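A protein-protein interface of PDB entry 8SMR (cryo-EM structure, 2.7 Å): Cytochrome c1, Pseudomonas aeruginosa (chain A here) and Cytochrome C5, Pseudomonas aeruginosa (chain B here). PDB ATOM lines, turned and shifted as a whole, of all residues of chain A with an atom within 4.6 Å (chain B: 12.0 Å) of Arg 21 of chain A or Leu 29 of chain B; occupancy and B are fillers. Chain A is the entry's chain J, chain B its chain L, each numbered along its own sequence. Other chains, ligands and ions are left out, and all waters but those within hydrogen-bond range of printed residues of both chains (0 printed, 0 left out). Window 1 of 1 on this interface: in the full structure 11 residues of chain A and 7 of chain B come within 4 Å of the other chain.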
ATOM      1  N   GLN A  17       2.793  13.095   8.951  1.00  0.00           N
ATOM      2  CA  GLN A  17       1.444  13.438   8.514  1.00  0.00           C
ATOM      3  C   GLN A  17       1.241  14.947   8.487  1.00  0.00           C
ATOM      4  O   GLN A  17       0.674  15.488   7.529  1.00  0.00           O
ATOM      5  CB  GLN A  17       0.419  12.778   9.434  1.00  0.00           C
ATOM      6  CG  GLN A  17       0.203  11.302   9.156  1.00  0.00           C
ATOM      7  CD  GLN A  17      -0.328  10.557  10.363  1.00  0.00           C
ATOM      8  OE1 GLN A  17      -0.868  11.160  11.290  1.00  0.00           O
ATOM      9  NE2 GLN A  17      -0.176   9.240  10.359  1.00  0.00           N
ATOM     10  N   ASP A  18       1.695  15.642   9.531  1.00  0.00           N
ATOM     11  CA  ASP A  18       1.596  17.098   9.534  1.00  0.00           C
ATOM     12  C   ASP A  18       2.422  17.699   8.404  1.00  0.00           C
ATOM     13  O   ASP A  18       1.993  18.656   7.749  1.00  0.00           O
ATOM     14  CB  ASP A  18       2.043  17.657  10.883  1.00  0.00           C
ATOM     15  CG  ASP A  18       1.932  19.167  10.952  1.00  0.00           C
ATOM     16  OD1 ASP A  18       0.820  19.691  10.740  1.00  0.00           O
ATOM     17  OD2 ASP A  18       2.957  19.830  11.217  1.00  0.00           O
ATOM     18  N   GLY A  19       3.608  17.146   8.157  1.00  0.00           N
ATOM     19  CA  GLY A  19       4.419  17.621   7.049  1.00  0.00           C
ATOM     20  C   GLY A  19       3.755  17.399   5.705  1.00  0.00           C
ATOM     21  O   GLY A  19       3.836  18.244   4.816  1.00  0.00           O
ATOM     22  N   ALA A  20       3.095  16.253   5.539  1.00  0.00           N
ATOM     23  CA  ALA A  20       2.384  15.973   4.298  1.00  0.00           C
ATOM     24  C   ALA A  20       1.215  16.930   4.111  1.00  0.00           C
ATOM     25  O   ALA A  20       0.949  17.380   2.995  1.00  0.00           O
ATOM     26  CB  ALA A  20       1.894  14.527   4.287  1.00  0.00           C
ATOM     27  N   ARG A  21       0.497  17.238   5.191  1.00  0.00           N
ATOM     28  CA  ARG A  21      -0.579  18.221   5.111  1.00  0.00           C
ATOM     29  C   ARG A  21      -0.036  19.586   4.706  1.00  0.00           C
ATOM     30  O   ARG A  21      -0.586  20.256   3.818  1.00  0.00           O
ATOM     31  CB  ARG A  21      -1.305  18.289   6.455  1.00  0.00           C
ATOM     32  CG  ARG A  21      -2.462  19.270   6.515  1.00  0.00           C
ATOM     33  CD  ARG A  21      -2.162  20.414   7.469  1.00  0.00           C
ATOM     34  NE  ARG A  21      -3.368  21.128   7.871  1.00  0.00           N
ATOM     35  CZ  ARG A  21      -3.371  22.292   8.505  1.00  0.00           C
ATOM     36  NH1 ARG A  21      -2.245  22.904   8.836  1.00  0.00           N
ATOM     37  NH2 ARG A  21      -4.533  22.857   8.819  1.00  0.00           N
ATOM     38  N   THR A  22       1.063  20.006   5.335  1.00  0.00           N
ATOM     39  CA  THR A  22       1.688  21.272   4.974  1.00  0.00           C
ATOM     40  C   THR A  22       2.114  21.275   3.512  1.00  0.00           C
ATOM     41  O   THR A  22       1.924  22.268   2.804  1.00  0.00           O
ATOM     42  CB  THR A  22       2.890  21.541   5.880  1.00  0.00           C
ATOM     43  OG1 THR A  22       2.473  21.523   7.251  1.00  0.00           O
ATOM     44  CG2 THR A  22       3.514  22.889   5.560  1.00  0.00           C
ATOM     45  N   PHE A  23       2.700  20.174   3.043  1.00  0.00           N
ATOM     46  CA  PHE A  23       3.135  20.102   1.655  1.00  0.00           C
ATOM     47  C   PHE A  23       1.947  20.159   0.701  1.00  0.00           C
ATOM     48  O   PHE A  23       1.993  20.847  -0.324  1.00  0.00           O
ATOM     49  CB  PHE A  23       3.945  18.825   1.428  1.00  0.00           C
ATOM     50  CG  PHE A  23       4.610  18.762   0.087  1.00  0.00           C
ATOM     51  CD1 PHE A  23       5.843  19.355  -0.115  1.00  0.00           C
ATOM     52  CD2 PHE A  23       4.005  18.113  -0.974  1.00  0.00           C
ATOM     53  CE1 PHE A  23       6.459  19.302  -1.346  1.00  0.00           C
ATOM     54  CE2 PHE A  23       4.617  18.058  -2.208  1.00  0.00           C
ATOM     55  CZ  PHE A  23       5.844  18.652  -2.395  1.00  0.00           C
ATOM     56  N   ALA A  24       0.870  19.444   1.023  1.00  0.00           N
ATOM     57  CA  ALA A  24      -0.281  19.401   0.132  1.00  0.00           C
ATOM     58  C   ALA A  24      -0.973  20.753   0.060  1.00  0.00           C
ATOM     59  O   ALA A  24      -1.554  21.105  -0.973  1.00  0.00           O
ATOM     60  CB  ALA A  24      -1.262  18.324   0.594  1.00  0.00           C
ATOM     61  N   ASN A  25      -0.926  21.526   1.146  1.00  0.00           N
ATOM     62  CA  ASN A  25      -1.662  22.787   1.174  1.00  0.00           C
ATOM     63  C   ASN A  25      -0.803  23.962   0.713  1.00  0.00           C
ATOM     64  O   ASN A  25      -1.168  24.679  -0.224  1.00  0.00           O
ATOM     65  CB  ASN A  25      -2.207  23.036   2.580  1.00  0.00           C
ATOM     66  CG  ASN A  25      -3.394  22.156   2.900  1.00  0.00           C
ATOM     67  OD1 ASN A  25      -4.527  22.471   2.543  1.00  0.00           O
ATOM     68  ND2 ASN A  25      -3.141  21.040   3.569  1.00  0.00           N
ATOM     69  N   ILE A  47      -1.716   6.688   6.792  1.00  0.00           N
ATOM     70  CA  ILE A  47      -2.957   7.408   6.523  1.00  0.00           C
ATOM     71  C   ILE A  47      -3.918   6.470   5.800  1.00  0.00           C
ATOM     72  O   ILE A  47      -3.535   5.860   4.792  1.00  0.00           O
ATOM     73  CB  ILE A  47      -2.699   8.679   5.699  1.00  0.00           C
ATOM     74  CG1 ILE A  47      -1.765   9.630   6.453  1.00  0.00           C
ATOM     75  CG2 ILE A  47      -4.010   9.379   5.382  1.00  0.00           C
ATOM     76  CD1 ILE A  47      -0.984  10.558   5.548  1.00  0.00           C
ATOM     77  N   LEU A  51      -8.954   8.594   3.822  1.00  0.00           N
ATOM     78  CA  LEU A  51      -8.505   9.833   4.448  1.00  0.00           C
ATOM     79  C   LEU A  51      -7.492  10.559   3.571  1.00  0.00           C
ATOM     80  O   LEU A  51      -7.545  11.787   3.440  1.00  0.00           O
ATOM     81  CB  LEU A  51      -7.910   9.533   5.822  1.00  0.00           C
ATOM     82  CG  LEU A  51      -8.114  10.618   6.874  1.00  0.00           C
ATOM     83  CD1 LEU A  51      -9.542  10.605   7.393  1.00  0.00           C
ATOM     84  CD2 LEU A  51      -7.124  10.431   8.007  1.00  0.00           C
ATOM     85  N   LYS A  55      -8.232  14.326   2.217  1.00  0.00           N
ATOM     86  CA  LYS A  55      -7.510  15.377   2.920  1.00  0.00           C
ATOM     87  C   LYS A  55      -6.271  15.885   2.201  1.00  0.00           C
ATOM     88  O   LYS A  55      -5.923  17.056   2.367  1.00  0.00           O
ATOM     89  CB  LYS A  55      -7.094  14.888   4.312  1.00  0.00           C
ATOM     90  CG  LYS A  55      -8.237  14.338   5.153  1.00  0.00           C
ATOM     91  CD  LYS A  55      -8.812  15.395   6.079  1.00  0.00           C
ATOM     92  CE  LYS A  55     -10.292  15.164   6.332  1.00  0.00           C
ATOM     93  NZ  LYS A  55     -10.755  15.809   7.590  1.00  0.00           N
ATOM     94  N   LEU A  56      -5.592  15.050   1.412  1.00  0.00           N
ATOM     95  CA  LEU A  56      -4.325  15.436   0.807  1.00  0.00           C
ATOM     96  C   LEU A  56      -4.337  15.469  -0.713  1.00  0.00           C
ATOM     97  O   LEU A  56      -3.474  16.131  -1.297  1.00  0.00           O
ATOM     98  CB  LEU A  56      -3.202  14.492   1.268  1.00  0.00           C
ATOM     99  CG  LEU A  56      -2.861  14.568   2.759  1.00  0.00           C
ATOM    100  CD1 LEU A  56      -1.868  13.487   3.150  1.00  0.00           C
ATOM    101  CD2 LEU A  56      -2.320  15.937   3.122  1.00  0.00           C
ATOM    102  N   LYS A 187       6.391  23.241  12.716  1.00  0.00           N
ATOM    103  CA  LYS A 187       5.758  23.103  11.407  1.00  0.00           C
ATOM    104  C   LYS A 187       6.798  22.818  10.330  1.00  0.00           C
ATOM    105  O   LYS A 187       6.641  21.895   9.518  1.00  0.00           O
ATOM    106  CB  LYS A 187       4.977  24.376  11.075  1.00  0.00           C
ATOM    107  CG  LYS A 187       4.123  24.298   9.816  1.00  0.00           C
ATOM    108  CD  LYS A 187       2.943  23.345   9.967  1.00  0.00           C
ATOM    109  CE  LYS A 187       1.905  23.881  10.943  1.00  0.00           C
ATOM    110  NZ  LYS A 187       0.696  23.015  11.012  1.00  0.00           N
ATOM    111  N   ALA B  24      -7.784  11.331  14.788  1.00  0.00           N
ATOM    112  CA  ALA B  24      -6.461  11.859  15.099  1.00  0.00           C
ATOM    113  C   ALA B  24      -5.715  12.215  13.819  1.00  0.00           C
ATOM    114  O   ALA B  24      -5.217  13.330  13.671  1.00  0.00           O
ATOM    115  CB  ALA B  24      -5.668  10.853  15.915  1.00  0.00           C
ATOM    116  N   ILE B  25      -5.636  11.257  12.894  1.00  0.00           N
ATOM    117  CA  ILE B  25      -5.016  11.531  11.602  1.00  0.00           C
ATOM    118  C   ILE B  25      -5.845  12.548  10.827  1.00  0.00           C
ATOM    119  O   ILE B  25      -5.301  13.458  10.191  1.00  0.00           O
ATOM    120  CB  ILE B  25      -4.829  10.228  10.802  1.00  0.00           C
ATOM    121  CG1 ILE B  25      -4.045   9.192  11.612  1.00  0.00           C
ATOM    122  CG2 ILE B  25      -4.094  10.505   9.497  1.00  0.00           C
ATOM    123  CD1 ILE B  25      -4.290   7.767  11.165  1.00  0.00           C
ATOM    124  N   ALA B  26      -7.173  12.412  10.868  1.00  0.00           N
ATOM    125  CA  ALA B  26      -8.036  13.318  10.118  1.00  0.00           C
ATOM    126  C   ALA B  26      -7.848  14.757  10.580  1.00  0.00           C
ATOM    127  O   ALA B  26      -7.745  15.678   9.759  1.00  0.00           O
ATOM    128  CB  ALA B  26      -9.496  12.892  10.270  1.00  0.00           C
ATOM    129  N   LYS B  27      -7.804  14.973  11.895  1.00  0.00           N
ATOM    130  CA  LYS B  27      -7.541  16.310  12.413  1.00  0.00           C
ATOM    131  C   LYS B  27      -6.159  16.791  11.992  1.00  0.00           C
ATOM    132  O   LYS B  27      -5.982  17.959  11.627  1.00  0.00           O
ATOM    133  CB  LYS B  27      -7.667  16.313  13.935  1.00  0.00           C
ATOM    134  CG  LYS B  27      -9.102  16.339  14.440  1.00  0.00           C
ATOM    135  CD  LYS B  27      -9.180  16.802  15.889  1.00  0.00           C
ATOM    136  CE  LYS B  27      -9.704  15.704  16.804  1.00  0.00           C
ATOM    137  NZ  LYS B  27      -8.635  14.740  17.184  1.00  0.00           N
ATOM    138  N   ARG B  28      -5.168  15.900  12.038  1.00  0.00           N
ATOM    139  CA  ARG B  28      -3.816  16.242  11.620  1.00  0.00           C
ATOM    140  C   ARG B  28      -3.753  16.639  10.151  1.00  0.00           C
ATOM    141  O   ARG B  28      -2.898  17.447   9.773  1.00  0.00           O
ATOM    142  CB  ARG B  28      -2.891  15.052  11.875  1.00  0.00           C
ATOM    143  CG  ARG B  28      -1.423  15.400  12.031  1.00  0.00           C
ATOM    144  CD  ARG B  28      -0.778  14.539  13.108  1.00  0.00           C
ATOM    145  NE  ARG B  28      -1.167  13.138  12.979  1.00  0.00           N
ATOM    146  CZ  ARG B  28      -1.537  12.352  13.982  1.00  0.00           C
ATOM    147  NH1 ARG B  28      -1.571  12.784  15.233  1.00  0.00           N
ATOM    148  NH2 ARG B  28      -1.885  11.094  13.724  1.00  0.00           N
ATOM    149  N   LEU B  29      -4.639  16.091   9.320  1.00  0.00           N
ATOM    150  CA  LEU B  29      -4.577  16.249   7.874  1.00  0.00           C
ATOM    151  C   LEU B  29      -5.583  17.268   7.345  1.00  0.00           C
ATOM    152  O   LEU B  29      -5.775  17.355   6.128  1.00  0.00           O
ATOM    153  CB  LEU B  29      -4.803  14.892   7.204  1.00  0.00           C
ATOM    154  CG  LEU B  29      -3.570  14.143   6.703  1.00  0.00           C
ATOM    155  CD1 LEU B  29      -2.504  14.054   7.781  1.00  0.00           C
ATOM    156  CD2 LEU B  29      -3.967  12.754   6.231  1.00  0.00           C
ATOM    157  N   GLU B  30      -6.213  18.041   8.218  1.00  0.00           N
ATOM    158  CA  GLU B  30      -7.273  18.944   7.793  1.00  0.00           C
ATOM    159  C   GLU B  30      -6.727  19.936   6.767  1.00  0.00           C
ATOM    160  O   GLU B  30      -5.662  20.526   6.997  1.00  0.00           O
ATOM    161  CB  GLU B  30      -7.834  19.699   9.000  1.00  0.00           C
ATOM    162  CG  GLU B  30      -9.118  19.142   9.634  1.00  0.00           C
ATOM    163  CD  GLU B  30     -10.293  18.984   8.678  1.00  0.00           C
ATOM    164  OE1 GLU B  30     -10.092  18.884   7.455  1.00  0.00           O
ATOM    165  OE2 GLU B  30     -11.443  18.952   9.168  1.00  0.00           O
ATOM    166  N   PRO B  31      -7.406  20.152   5.637  1.00  0.00           N
ATOM    167  CA  PRO B  31      -6.917  21.153   4.681  1.00  0.00           C
ATOM    168  C   PRO B  31      -6.894  22.547   5.289  1.00  0.00           C
ATOM    169  O   PRO B  31      -7.725  22.901   6.128  1.00  0.00           O
ATOM    170  CB  PRO B  31      -7.918  21.063   3.522  1.00  0.00           C
ATOM    171  CG  PRO B  31      -8.526  19.721   3.646  1.00  0.00           C
ATOM    172  CD  PRO B  31      -8.581  19.438   5.110  1.00  0.00           C
ATOM    173  N   VAL B  32      -5.916  23.342   4.851  1.00  0.00           N
ATOM    174  CA  VAL B  32      -5.747  24.685   5.395  1.00  0.00           C
ATOM    175  C   VAL B  32      -6.924  25.573   5.009  1.00  0.00           C
ATOM    176  O   VAL B  32      -7.481  26.288   5.850  1.00  0.00           O
ATOM    177  CB  VAL B  32      -4.412  25.282   4.918  1.00  0.00           C
ATOM    178  CG1 VAL B  32      -4.327  26.761   5.272  1.00  0.00           C
ATOM    179  CG2 VAL B  32      -3.248  24.517   5.520  1.00  0.00           C
ATOM    180  N   GLY B  33      -7.321  25.543   3.740  1.00  0.00           N
ATOM    181  CA  GLY B  33      -8.361  26.433   3.262  1.00  0.00           C
ATOM    182  C   GLY B  33      -9.724  26.025   3.784  1.00  0.00           C
ATOM    183  O   GLY B  33     -10.192  24.908   3.510  1.00  0.00           O
ATOM    184  N   LYS B  34     -10.374  26.911   4.532  1.00  0.00           N
ATOM    185  CA  LYS B  34     -11.733  26.702   5.005  1.00  0.00           C
ATOM    186  C   LYS B  34     -12.684  27.582   4.205  1.00  0.00           C
ATOM    187  O   LYS B  34     -12.435  28.777   4.023  1.00  0.00           O
ATOM    188  CB  LYS B  34     -11.855  27.026   6.496  1.00  0.00           C
ATOM    189  CG  LYS B  34     -10.904  26.247   7.393  1.00  0.00           C
ATOM    190  CD  LYS B  34     -11.540  24.966   7.916  1.00  0.00           C
ATOM    191  CE  LYS B  34     -10.573  23.794   7.844  1.00  0.00           C
ATOM    192  NZ  LYS B  34     -10.456  23.246   6.465  1.00  0.00           N
ATOM    193  N   VAL B  35     -13.773  26.985   3.726  1.00  0.00           N
ATOM    194  CA  VAL B  35     -14.753  27.677   2.898  1.00  0.00           C
ATOM    195  C   VAL B  35     -16.065  27.749   3.663  1.00  0.00           C
ATOM    196  O   VAL B  35     -16.558  26.730   4.161  1.00  0.00           O
ATOM    197  CB  VAL B  35     -14.947  26.978   1.539  1.00  0.00           C
ATOM    198  CG1 VAL B  35     -15.540  25.588   1.722  1.00  0.00           C
ATOM    199  CG2 VAL B  35     -15.824  27.825   0.626  1.00  0.00           C
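NE of Arg 28 of chain B sits at hydrogen-bond distance from OE1 of Gln 17 of chain A. O of Glu 30 of chain B lies within hydrogen-bond range of NE of Arg 21 of chain A (2.5 Å). OD1 of Asn 25 of chain A lies within hydrogen-bond range of N of Val 32 of chain B. OE1 of Glu 30 of chain B lies within salt-bridge range of NZ of Lys 55 of chain A (3.1 Å).
ND2 of Asn 25 of chain A is in hydrogen-bond range of O of Arg 21 of chain A (2.7 Å). The backbone carbonyl oxygen of Pro 31 of chain B sits at hydrogen-bond distance from the side-chain amino group of Lys 34 of chain B, 2.8 Å away.
Among the printed residues, merely in contact across the chains: Lys 55 of chain A with Leu 29 of chain B, Leu 51 of chain A with Ile 25 of chain B, Asn 25 of chain A with Pro 31 of chain B, Leu 51 of chain A with Ala 26 of chain B, Ile 47 of chain A with Leu 29 of chain B, Gln 17 of chain A with Leu 29 of chain B, Lys 55 of chain A with Ala 26 of chain B, Arg 21 of chain A with Val 32 of chain B, Gln 17 of chain A with Ile 25 of chain B, Arg 21 of chain A with Arg 28 of chain B, Leu 56 of chain A with Leu 29 of chain B, Arg 21 of chain A with Leu 29 of chain B, Ile 47 of chain A with Ile 25 of chain B and Lys 55 of chain A with Pro 31 of chain B.
Arg 21 of chain A touches just these residues of chain B: Arg 28, Leu 29, Glu 30 and Val 32. Of chain A, only Gln 17, Arg 21, Ile 47, Lys 55 and Leu 56 come within 4 Å of Leu 29 of chain B. No residue of chain B comes within 4 Å of Gly 19 of chain A. No residue of chain B comes within 4 Å of Ala 20 of chain A. No residue of chain B comes within 4 Å of Thr 22 of chain A. No residue of chain B comes within 4 Å of Ala 24 of chain A. Asn 25 of chain A touches just these residues of chain B: Pro 31 and Val 32. Of chain B, only Ile 25 (3.9 Å) and Leu 29 (3.5 Å) come within 4 Å of Ile 47 of chain A. Leu 51 of chain A touches two residues of chain B. Of the printed residues of chain B, Lys 55 of chain A touches Ala 26, Leu 29, Glu 30 and Pro 31. Leu 56 of chain A touches one residue of chain B. Printed residues of chain A within 4 Å of Val 32 of chain B: Arg 21 and Asn 25. Printed residues of chain A within 4 Å of Pro 31 of chain B: Asn 25 (3.5 Å) and Lys 55 (3.9 Å). Printed residues of chain A within 4 Å of Ile 25 of chain B: Gln 17, Ile 47 and Leu 51. The nearest printed residue of chain A that does not touch Glu 30 of chain B is Asn 25 of chain A (4.3 Å).
Of the 14 printed residues of chain A, 7 touch a printed residue of chain B. Hydrophobic or aromatic side chains of chain A within 4 Å of the printed part of chain B: Ile 47, Leu 51 and Leu 56. Printed residues of chain B that touch a printed residue of chain A: Ile 25, Ala 26, Arg 28, Leu 29, Glu 30, Pro 31 and Val 32. Along chain B the printed residues that touch a printed residue of chain A span positions 25 to 32. Among the printed residues, 18 pairs touch across the chains.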
